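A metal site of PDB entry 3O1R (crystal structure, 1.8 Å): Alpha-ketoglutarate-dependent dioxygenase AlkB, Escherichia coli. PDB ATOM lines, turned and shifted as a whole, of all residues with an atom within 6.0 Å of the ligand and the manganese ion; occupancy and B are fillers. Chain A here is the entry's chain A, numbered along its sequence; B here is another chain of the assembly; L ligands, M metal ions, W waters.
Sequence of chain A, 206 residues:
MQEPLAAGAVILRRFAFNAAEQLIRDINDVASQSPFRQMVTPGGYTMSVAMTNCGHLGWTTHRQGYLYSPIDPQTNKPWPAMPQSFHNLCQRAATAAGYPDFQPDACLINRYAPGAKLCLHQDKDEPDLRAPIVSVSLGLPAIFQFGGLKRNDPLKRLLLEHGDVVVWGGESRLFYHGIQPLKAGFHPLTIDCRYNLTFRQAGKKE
The side-chain amide oxygen (OD1) of Asn 110 sits close to an oxygen (O1) of the ligand.
NH2 of Arg 200 lies within salt-bridge range of O1 of the ligand, 3.7 Å away.
An oxygen (O5) of the ligand lies within salt-bridge range of the guanidinium group (NH2) of Arg 194 (2.9 Å).
O4 of the ligand lies within hydrogen-bond range of OH of Tyr 112.
O5 of the ligand is in hydrogen-bond range of ND2 of Asn 196, 3.2 Å away.
The side-chain carboxylate (OD2) of Asp 123 is in salt-bridge range of the guanidinium group (NE) of Arg 200.
The backbone carbonyl oxygen (O) of Leu 108 sits at hydrogen-bond distance from the backbone NH (N) of Thr 198, at 2.9 Å.
The backbone NH of Tyr 112 is in hydrogen-bond range of the backbone carbonyl oxygen of Arg 194 (2.8 Å).
OG1 of Thr 198 is in hydrogen-bond range of OD1 of Asn 196 (2.7 Å).
O of Asn 110 sits at hydrogen-bond distance from N of Asn 196 (2.8 Å).
The backbone NH of Ile 179 sits at hydrogen-bond distance from the backbone carbonyl oxygen of Leu 118, at 2.9 Å.
OG of Ser 137 lies within hydrogen-bond range of NH2 of Arg 194 (2.7 Å).
The side-chain amide nitrogen of Asn 196 sits at hydrogen-bond distance from the side-chain hydroxyl of Ser 135, at 2.7 Å.
Residues that only touch the ligand: MDK 7 of chain B (3.4 Å), Ile 179 (3.4 Å), Leu 118 (3.5 Å), Ser 135 (3.7 Å), Leu 108 (3.8 Å) and Thr 198 (3.8 Å).
Hydrophobic or aromatic side chains that line the ligand: Leu 108, Tyr 112, Leu 118, His 121, His 177 and Ile 179.
The nearest printed residue that does not touch the ligand is Phe 144 (4.3 Å).
Three residues have an atom within 4 Å of the manganese ion: His 121, Asp 123 and His 177.
The manganese ion is bound by O2 of the ligand (2.1 Å), NE2 of His 177 (2.1 Å), NE2 of His 121 (2.2 Å), O3 of the ligand (2.2 Å), OD1 of Asp 123 (2.2 Å) and water W4 (2.4 Å).
The manganese ion has six donor atoms within binding distance.
Water W4 lies within hydrogen-bond range of OD2 of Asp 123 (2.5 Å) and NH2 of Arg 200 (3.4 Å).
Water W2 lies within hydrogen-bond range of O5 of the ligand (2.6 Å) and OG of Ser 135 (2.8 Å).
Water W1 lies within hydrogen-bond range of an oxygen (O1) of the ligand (2.6 Å), O2 of MDK 7 of chain B (2.7 Å) and the side-chain amide oxygen of Asn 110 (3.3 Å).
Water W3 lies within hydrogen-bond range of OG1 of Thr 198 (2.6 Å) and OG of Ser 135 (3.1 Å).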
ATOM      1  N   MET A  51     -16.347 -11.497  -3.422  1.00  0.00           N
ATOM      2  CA  MET A  51     -16.423 -12.179  -4.732  1.00  0.00           C
ATOM      3  C   MET A  51     -15.461 -11.606  -5.750  1.00  0.00           C
ATOM      4  O   MET A  51     -15.027 -10.446  -5.662  1.00  0.00           O
ATOM      5  CB  MET A  51     -17.792 -11.967  -5.362  1.00  0.00           C
ATOM      6  CG  MET A  51     -18.896 -12.641  -4.656  1.00  0.00           C
ATOM      7  SD  MET A  51     -20.513 -12.085  -5.322  1.00  0.00           S
ATOM      8  CE  MET A  51     -21.444 -13.399  -4.566  1.00  0.00           C
ATOM      9  N   LEU A 108     -17.784 -17.481 -11.170  1.00  0.00           N
ATOM     10  CA  LEU A 108     -17.904 -16.547 -10.045  1.00  0.00           C
ATOM     11  C   LEU A 108     -17.226 -17.190  -8.868  1.00  0.00           C
ATOM     12  O   LEU A 108     -17.544 -18.330  -8.555  1.00  0.00           O
ATOM     13  CB  LEU A 108     -19.386 -16.297  -9.752  1.00  0.00           C
ATOM     14  CG  LEU A 108     -19.732 -15.490  -8.467  1.00  0.00           C
ATOM     15  CD1 LEU A 108     -19.113 -14.114  -8.493  1.00  0.00           C
ATOM     16  CD2 LEU A 108     -21.221 -15.366  -8.298  1.00  0.00           C
ATOM     17  N   ASN A 110     -16.567 -17.118  -4.986  1.00  0.00           N
ATOM     18  CA  ASN A 110     -17.047 -16.618  -3.682  1.00  0.00           C
ATOM     19  C   ASN A 110     -16.104 -17.014  -2.566  1.00  0.00           C
ATOM     20  O   ASN A 110     -15.656 -18.166  -2.517  1.00  0.00           O
ATOM     21  CB  ASN A 110     -18.371 -17.287  -3.334  1.00  0.00           C
ATOM     22  CG  ASN A 110     -19.533 -16.706  -4.109  1.00  0.00           C
ATOM     23  OD1 ASN A 110     -20.598 -17.297  -4.168  1.00  0.00           O
ATOM     24  ND2 ASN A 110     -19.338 -15.556  -4.699  1.00  0.00           N
ATOM     25  N   TYR A 112     -15.971 -17.074   1.615  1.00  0.00           N
ATOM     26  CA  TYR A 112     -16.703 -16.980   2.878  1.00  0.00           C
ATOM     27  C   TYR A 112     -15.738 -16.879   4.061  1.00  0.00           C
ATOM     28  O   TYR A 112     -14.952 -17.805   4.334  1.00  0.00           O
ATOM     29  CB  TYR A 112     -17.549 -18.233   3.065  1.00  0.00           C
ATOM     30  CG  TYR A 112     -18.652 -18.377   2.066  1.00  0.00           C
ATOM     31  CD1 TYR A 112     -18.394 -18.805   0.765  1.00  0.00           C
ATOM     32  CD2 TYR A 112     -19.967 -18.120   2.432  1.00  0.00           C
ATOM     33  CE1 TYR A 112     -19.486 -18.942  -0.183  1.00  0.00           C
ATOM     34  CE2 TYR A 112     -20.996 -18.255   1.544  1.00  0.00           C
ATOM     35  CZ  TYR A 112     -20.737 -18.669   0.244  1.00  0.00           C
ATOM     36  OH  TYR A 112     -21.782 -18.798  -0.628  1.00  0.00           O
ATOM     37  N   LEU A 118     -25.174 -16.927   2.170  1.00  0.00           N
ATOM     38  CA  LEU A 118     -25.874 -16.519   0.999  1.00  0.00           C
ATOM     39  C   LEU A 118     -27.326 -16.926   1.161  1.00  0.00           C
ATOM     40  O   LEU A 118     -27.641 -18.120   1.168  1.00  0.00           O
ATOM     41  CB  LEU A 118     -25.317 -17.250  -0.218  1.00  0.00           C
ATOM     42  CG  LEU A 118     -25.355 -16.600  -1.564  1.00  0.00           C
ATOM     43  CD1 LEU A 118     -24.750 -15.152  -1.535  1.00  0.00           C
ATOM     44  CD2 LEU A 118     -24.597 -17.513  -2.587  1.00  0.00           C
ATOM     45  N   HIS A 121     -31.661 -18.104  -2.987  1.00  0.00           N
ATOM     46  CA  HIS A 121     -31.806 -17.347  -4.229  1.00  0.00           C
ATOM     47  C   HIS A 121     -31.859 -18.338  -5.374  1.00  0.00           C
ATOM     48  O   HIS A 121     -31.588 -19.550  -5.206  1.00  0.00           O
ATOM     49  CB  HIS A 121     -30.636 -16.378  -4.435  1.00  0.00           C
ATOM     50  CG  HIS A 121     -29.324 -17.064  -4.636  1.00  0.00           C
ATOM     51  ND1 HIS A 121     -28.607 -17.585  -3.593  1.00  0.00           N
ATOM     52  CD2 HIS A 121     -28.622 -17.373  -5.763  1.00  0.00           C
ATOM     53  CE1 HIS A 121     -27.516 -18.173  -4.043  1.00  0.00           C
ATOM     54  NE2 HIS A 121     -27.492 -18.048  -5.353  1.00  0.00           N
ATOM     55  N   GLN A 122     -32.264 -17.830  -6.538  1.00  0.00           N
ATOM     56  CA  GLN A 122     -32.202 -18.617  -7.767  1.00  0.00           C
ATOM     57  C   GLN A 122     -31.123 -18.014  -8.638  1.00  0.00           C
ATOM     58  O   GLN A 122     -30.929 -16.794  -8.610  1.00  0.00           O
ATOM     59  CB  GLN A 122     -33.521 -18.515  -8.518  1.00  0.00           C
ATOM     60  CG  GLN A 122     -34.714 -19.086  -7.779  1.00  0.00           C
ATOM     61  CD  GLN A 122     -36.010 -18.775  -8.499  1.00  0.00           C
ATOM     62  OE1 GLN A 122     -36.397 -17.618  -8.615  1.00  0.00           O
ATOM     63  NE2 GLN A 122     -36.683 -19.818  -9.021  1.00  0.00           N
ATOM     64  N   ASP A 123     -30.476 -18.846  -9.454  1.00  0.00           N
ATOM     65  CA  ASP A 123     -29.558 -18.341 -10.467  1.00  0.00           C
ATOM     66  C   ASP A 123     -30.365 -18.150 -11.730  1.00  0.00           C
ATOM     67  O   ASP A 123     -30.605 -19.105 -12.449  1.00  0.00           O
ATOM     68  CB  ASP A 123     -28.467 -19.340 -10.780  1.00  0.00           C
ATOM     69  CG  ASP A 123     -27.426 -19.458  -9.711  1.00  0.00           C
ATOM     70  OD1 ASP A 123     -27.652 -19.100  -8.557  1.00  0.00           O
ATOM     71  OD2 ASP A 123     -26.355 -19.961 -10.037  1.00  0.00           O
ATOM     72  N   SER A 135     -20.825 -26.238  -9.213  1.00  0.00           N
ATOM     73  CA  SER A 135     -20.456 -25.498  -8.009  1.00  0.00           C
ATOM     74  C   SER A 135     -19.433 -26.320  -7.234  1.00  0.00           C
ATOM     75  O   SER A 135     -19.725 -27.415  -6.789  1.00  0.00           O
ATOM     76  CB  SER A 135     -21.695 -25.256  -7.131  1.00  0.00           C
ATOM     77  OG  SER A 135     -21.347 -24.463  -5.993  1.00  0.00           O
ATOM     78  N   SER A 137     -16.661 -26.664  -4.022  1.00  0.00           N
ATOM     79  CA  SER A 137     -16.461 -26.156  -2.644  1.00  0.00           C
ATOM     80  C   SER A 137     -15.030 -26.417  -2.279  1.00  0.00           C
ATOM     81  O   SER A 137     -14.516 -27.507  -2.574  1.00  0.00           O
ATOM     82  CB  SER A 137     -17.342 -26.919  -1.641  1.00  0.00           C
ATOM     83  OG  SER A 137     -18.726 -26.584  -1.785  1.00  0.00           O
ATOM     84  N   PHE A 144     -25.331 -26.264   2.826  1.00  0.00           N
ATOM     85  CA  PHE A 144     -25.933 -25.861   1.580  1.00  0.00           C
ATOM     86  C   PHE A 144     -27.407 -26.215   1.677  1.00  0.00           C
ATOM     87  O   PHE A 144     -27.762 -27.327   2.061  1.00  0.00           O
ATOM     88  CB  PHE A 144     -25.245 -26.620   0.457  1.00  0.00           C
ATOM     89  CG  PHE A 144     -25.792 -26.344  -0.932  1.00  0.00           C
ATOM     90  CD1 PHE A 144     -25.644 -25.090  -1.532  1.00  0.00           C
ATOM     91  CD2 PHE A 144     -26.379 -27.389  -1.657  1.00  0.00           C
ATOM     92  CE1 PHE A 144     -26.062 -24.885  -2.833  1.00  0.00           C
ATOM     93  CE2 PHE A 144     -26.806 -27.183  -2.961  1.00  0.00           C
ATOM     94  CZ  PHE A 144     -26.675 -25.942  -3.554  1.00  0.00           C
ATOM     95  N   LEU A 160     -21.386 -29.356   2.750  1.00  0.00           N
ATOM     96  CA  LEU A 160     -20.480 -29.399   1.607  1.00  0.00           C
ATOM     97  C   LEU A 160     -19.063 -29.266   2.146  1.00  0.00           C
ATOM     98  O   LEU A 160     -18.717 -28.302   2.850  1.00  0.00           O
ATOM     99  CB  LEU A 160     -20.799 -28.294   0.595  1.00  0.00           C
ATOM    100  CG  LEU A 160     -22.161 -28.335  -0.073  1.00  0.00           C
ATOM    101  CD1 LEU A 160     -22.190 -27.211  -1.120  1.00  0.00           C
ATOM    102  CD2 LEU A 160     -22.315 -29.698  -0.780  1.00  0.00           C
ATOM    103  N   TRP A 168     -26.371 -28.712 -10.780  1.00  0.00           N
ATOM    104  CA  TRP A 168     -27.814 -28.742 -10.994  1.00  0.00           C
ATOM    105  C   TRP A 168     -28.195 -28.161 -12.350  1.00  0.00           C
ATOM    106  O   TRP A 168     -27.464 -27.307 -12.922  1.00  0.00           O
ATOM    107  CB  TRP A 168     -28.612 -28.116  -9.831  1.00  0.00           C
ATOM    108  CG  TRP A 168     -28.360 -26.654  -9.559  1.00  0.00           C
ATOM    109  CD1 TRP A 168     -29.146 -25.595  -9.975  1.00  0.00           C
ATOM    110  CD2 TRP A 168     -27.326 -26.102  -8.743  1.00  0.00           C
ATOM    111  NE1 TRP A 168     -28.629 -24.415  -9.484  1.00  0.00           N
ATOM    112  CE2 TRP A 168     -27.505 -24.697  -8.735  1.00  0.00           C
ATOM    113  CE3 TRP A 168     -26.260 -26.649  -8.015  1.00  0.00           C
ATOM    114  CZ2 TRP A 168     -26.665 -23.837  -8.042  1.00  0.00           C
ATOM    115  CZ3 TRP A 168     -25.417 -25.795  -7.329  1.00  0.00           C
ATOM    116  CH2 TRP A 168     -25.613 -24.398  -7.361  1.00  0.00           C
ATOM    117  N   HIS A 177     -31.578 -22.052  -3.616  1.00  0.00           N
ATOM    118  CA  HIS A 177     -30.477 -22.621  -2.898  1.00  0.00           C
ATOM    119  C   HIS A 177     -29.725 -21.543  -2.137  1.00  0.00           C
ATOM    120  O   HIS A 177     -29.851 -20.346  -2.421  1.00  0.00           O
ATOM    121  CB  HIS A 177     -29.535 -23.381  -3.872  1.00  0.00           C
ATOM    122  CG  HIS A 177     -28.944 -22.491  -4.928  1.00  0.00           C
ATOM    123  ND1 HIS A 177     -29.630 -22.132  -6.067  1.00  0.00           N
ATOM    124  CD2 HIS A 177     -27.761 -21.831  -4.973  1.00  0.00           C
ATOM    125  CE1 HIS A 177     -28.883 -21.303  -6.789  1.00  0.00           C
ATOM    126  NE2 HIS A 177     -27.742 -21.108  -6.148  1.00  0.00           N
ATOM    127  N   GLY A 178     -28.930 -21.938  -1.163  1.00  0.00           N
ATOM    128  CA  GLY A 178     -28.202 -20.948  -0.375  1.00  0.00           C
ATOM    129  C   GLY A 178     -27.169 -21.591   0.508  1.00  0.00           C
ATOM    130  O   GLY A 178     -27.001 -22.837   0.495  1.00  0.00           O
ATOM    131  N   ILE A 179     -26.478 -20.750   1.265  1.00  0.00           N
ATOM    132  CA  ILE A 179     -25.449 -21.157   2.200  1.00  0.00           C
ATOM    133  C   ILE A 179     -25.736 -20.551   3.569  1.00  0.00           C
ATOM    134  O   ILE A 179     -25.967 -19.323   3.699  1.00  0.00           O
ATOM    135  CB  ILE A 179     -24.046 -20.759   1.690  1.00  0.00           C
ATOM    136  CG1 ILE A 179     -23.735 -21.523   0.370  1.00  0.00           C
ATOM    137  CG2 ILE A 179     -22.947 -21.037   2.754  1.00  0.00           C
ATOM    138  CD1 ILE A 179     -23.404 -22.995   0.577  1.00  0.00           C
ATOM    139  N   ARG A 194     -13.775 -20.485   3.379  1.00  0.00           N
ATOM    140  CA  ARG A 194     -14.306 -21.374   2.361  1.00  0.00           C
ATOM    141  C   ARG A 194     -14.244 -20.600   1.048  1.00  0.00           C
ATOM    142  O   ARG A 194     -14.527 -19.399   1.037  1.00  0.00           O
ATOM    143  CB  ARG A 194     -15.773 -21.714   2.679  1.00  0.00           C
ATOM    144  CG  ARG A 194     -16.483 -22.549   1.557  1.00  0.00           C
ATOM    145  CD  ARG A 194     -17.926 -22.934   1.935  1.00  0.00           C
ATOM    146  NE  ARG A 194     -18.496 -23.788   0.888  1.00  0.00           N
ATOM    147  CZ  ARG A 194     -19.373 -23.388  -0.020  1.00  0.00           C
ATOM    148  NH1 ARG A 194     -19.829 -22.124  -0.046  1.00  0.00           N
ATOM    149  NH2 ARG A 194     -19.799 -24.254  -0.944  1.00  0.00           N
ATOM    150  N   ASN A 196     -15.888 -20.938  -3.011  1.00  0.00           N
ATOM    151  CA  ASN A 196     -16.772 -21.645  -3.917  1.00  0.00           C
ATOM    152  C   ASN A 196     -16.585 -21.123  -5.341  1.00  0.00           C
ATOM    153  O   ASN A 196     -16.498 -19.915  -5.554  1.00  0.00           O
ATOM    154  CB  ASN A 196     -18.223 -21.476  -3.464  1.00  0.00           C
ATOM    155  CG  ASN A 196     -19.220 -22.040  -4.475  1.00  0.00           C
ATOM    156  OD1 ASN A 196     -19.780 -21.293  -5.256  1.00  0.00           O
ATOM    157  ND2 ASN A 196     -19.432 -23.336  -4.457  1.00  0.00           N
ATOM    158  N   THR A 198     -18.348 -21.075  -8.956  1.00  0.00           N
ATOM    159  CA  THR A 198     -19.605 -21.375  -9.612  1.00  0.00           C
ATOM    160  C   THR A 198     -19.499 -21.086 -11.117  1.00  0.00           C
ATOM    161  O   THR A 198     -19.407 -19.909 -11.533  1.00  0.00           O
ATOM    162  CB  THR A 198     -20.771 -20.543  -9.015  1.00  0.00           C
ATOM    163  OG1 THR A 198     -21.012 -21.000  -7.678  1.00  0.00           O
ATOM    164  CG2 THR A 198     -22.001 -20.854  -9.815  1.00  0.00           C
ATOM    165  N   ARG A 200     -20.776 -21.071 -15.012  1.00  0.00           N
ATOM    166  CA  ARG A 200     -22.018 -20.873 -15.712  1.00  0.00           C
ATOM    167  C   ARG A 200     -21.768 -20.620 -17.182  1.00  0.00           C
ATOM    168  O   ARG A 200     -20.699 -20.156 -17.583  1.00  0.00           O
ATOM    169  CB  ARG A 200     -22.761 -19.644 -15.147  1.00  0.00           C
ATOM    170  CG  ARG A 200     -23.023 -19.645 -13.626  1.00  0.00           C
ATOM    171  CD  ARG A 200     -24.008 -18.526 -13.247  1.00  0.00           C
ATOM    172  NE  ARG A 200     -24.405 -18.506 -11.814  1.00  0.00           N
ATOM    173  CZ  ARG A 200     -23.632 -18.073 -10.830  1.00  0.00           C
ATOM    174  NH1 ARG A 200     -22.425 -17.646 -11.128  1.00  0.00           N
ATOM    175  NH2 ARG A 200     -24.033 -18.083  -9.549  1.00  0.00           N
ATOM    176  P   MDK B   7     -32.208 -12.509  -4.006  1.00  0.00           P
ATOM    177  N1  MDK B   7     -27.538 -13.634  -5.087  1.00  0.00           N
ATOM    178  C2  MDK B   7     -26.398 -14.091  -5.743  1.00  0.00           C
ATOM    179  O2  MDK B   7     -25.317 -14.106  -5.102  1.00  0.00           O
ATOM    180  C3  MDK B   7     -26.481 -14.500  -7.060  1.00  0.00           C
ATOM    181  C4  MDK B   7     -27.701 -14.468  -7.705  1.00  0.00           C
ATOM    182  N4  MDK B   7     -27.814 -14.888  -8.981  1.00  0.00           N
ATOM    183  C5  MDK B   7     -28.830 -14.028  -7.030  1.00  0.00           C
ATOM    184  C6  MDK B   7     -28.725 -13.614  -5.711  1.00  0.00           C
ATOM    185  C1' MDK B   7     -27.445 -13.266  -3.677  1.00  0.00           C
ATOM    186  O1P MDK B   7     -31.993 -11.869  -5.359  1.00  0.00           O
ATOM    187  C2' MDK B   7     -27.849 -11.828  -3.361  1.00  0.00           C
ATOM    188  C21 MDK B   7     -25.285 -15.014  -7.813  1.00  0.00           C
ATOM    189  O2P MDK B   7     -32.755 -13.912  -4.029  1.00  0.00           O
ATOM    190  C3' MDK B   7     -28.357 -11.980  -1.924  1.00  0.00           C
ATOM    191  O3' MDK B   7     -27.189 -11.975  -1.042  1.00  0.00           O
ATOM    192  C4' MDK B   7     -29.018 -13.353  -1.901  1.00  0.00           C
ATOM    193  O4' MDK B   7     -28.436 -14.076  -3.021  1.00  0.00           O
ATOM    194  C5' MDK B   7     -30.531 -13.269  -2.072  1.00  0.00           C
ATOM    195  O5' MDK B   7     -30.781 -12.458  -3.231  1.00  0.00           O
HETATM  196  C1  LIG L   1     -23.896 -18.608  -6.133  1.00  0.00           C
HETATM  197  O1  LIG L   1     -22.801 -18.003  -6.090  1.00  0.00           O
HETATM  198  O2  LIG L   1     -24.822 -18.285  -6.923  1.00  0.00           O
HETATM  199  C2  LIG L   1     -24.103 -19.748  -5.230  1.00  0.00           C
HETATM  200  O3  LIG L   1     -25.200 -20.304  -5.152  1.00  0.00           O
HETATM  201  C3  LIG L   1     -22.935 -20.245  -4.444  1.00  0.00           C
HETATM  202  C4  LIG L   1     -23.277 -21.543  -3.732  1.00  0.00           C
HETATM  203  C5  LIG L   1     -22.122 -21.940  -2.834  1.00  0.00           C
HETATM  204  O4  LIG L   1     -21.334 -21.068  -2.426  1.00  0.00           O
HETATM  205  O5  LIG L   1     -21.990 -23.165  -2.550  1.00  0.00           O
HETATM  206 MN    MN M   1     -26.502 -19.451  -6.680  1.00  0.00          MN
HETATM  207  O   HOH W   1     -23.070 -15.505  -5.369  1.00  0.00           O
HETATM  208  O   HOH W   2     -22.865 -25.223  -3.796  1.00  0.00           O
HETATM  209  O   HOH W   3     -23.221 -22.122  -6.949  1.00  0.00           O
HETATM  210  O   HOH W   4     -25.189 -20.851  -8.045  1.00  0.00           O
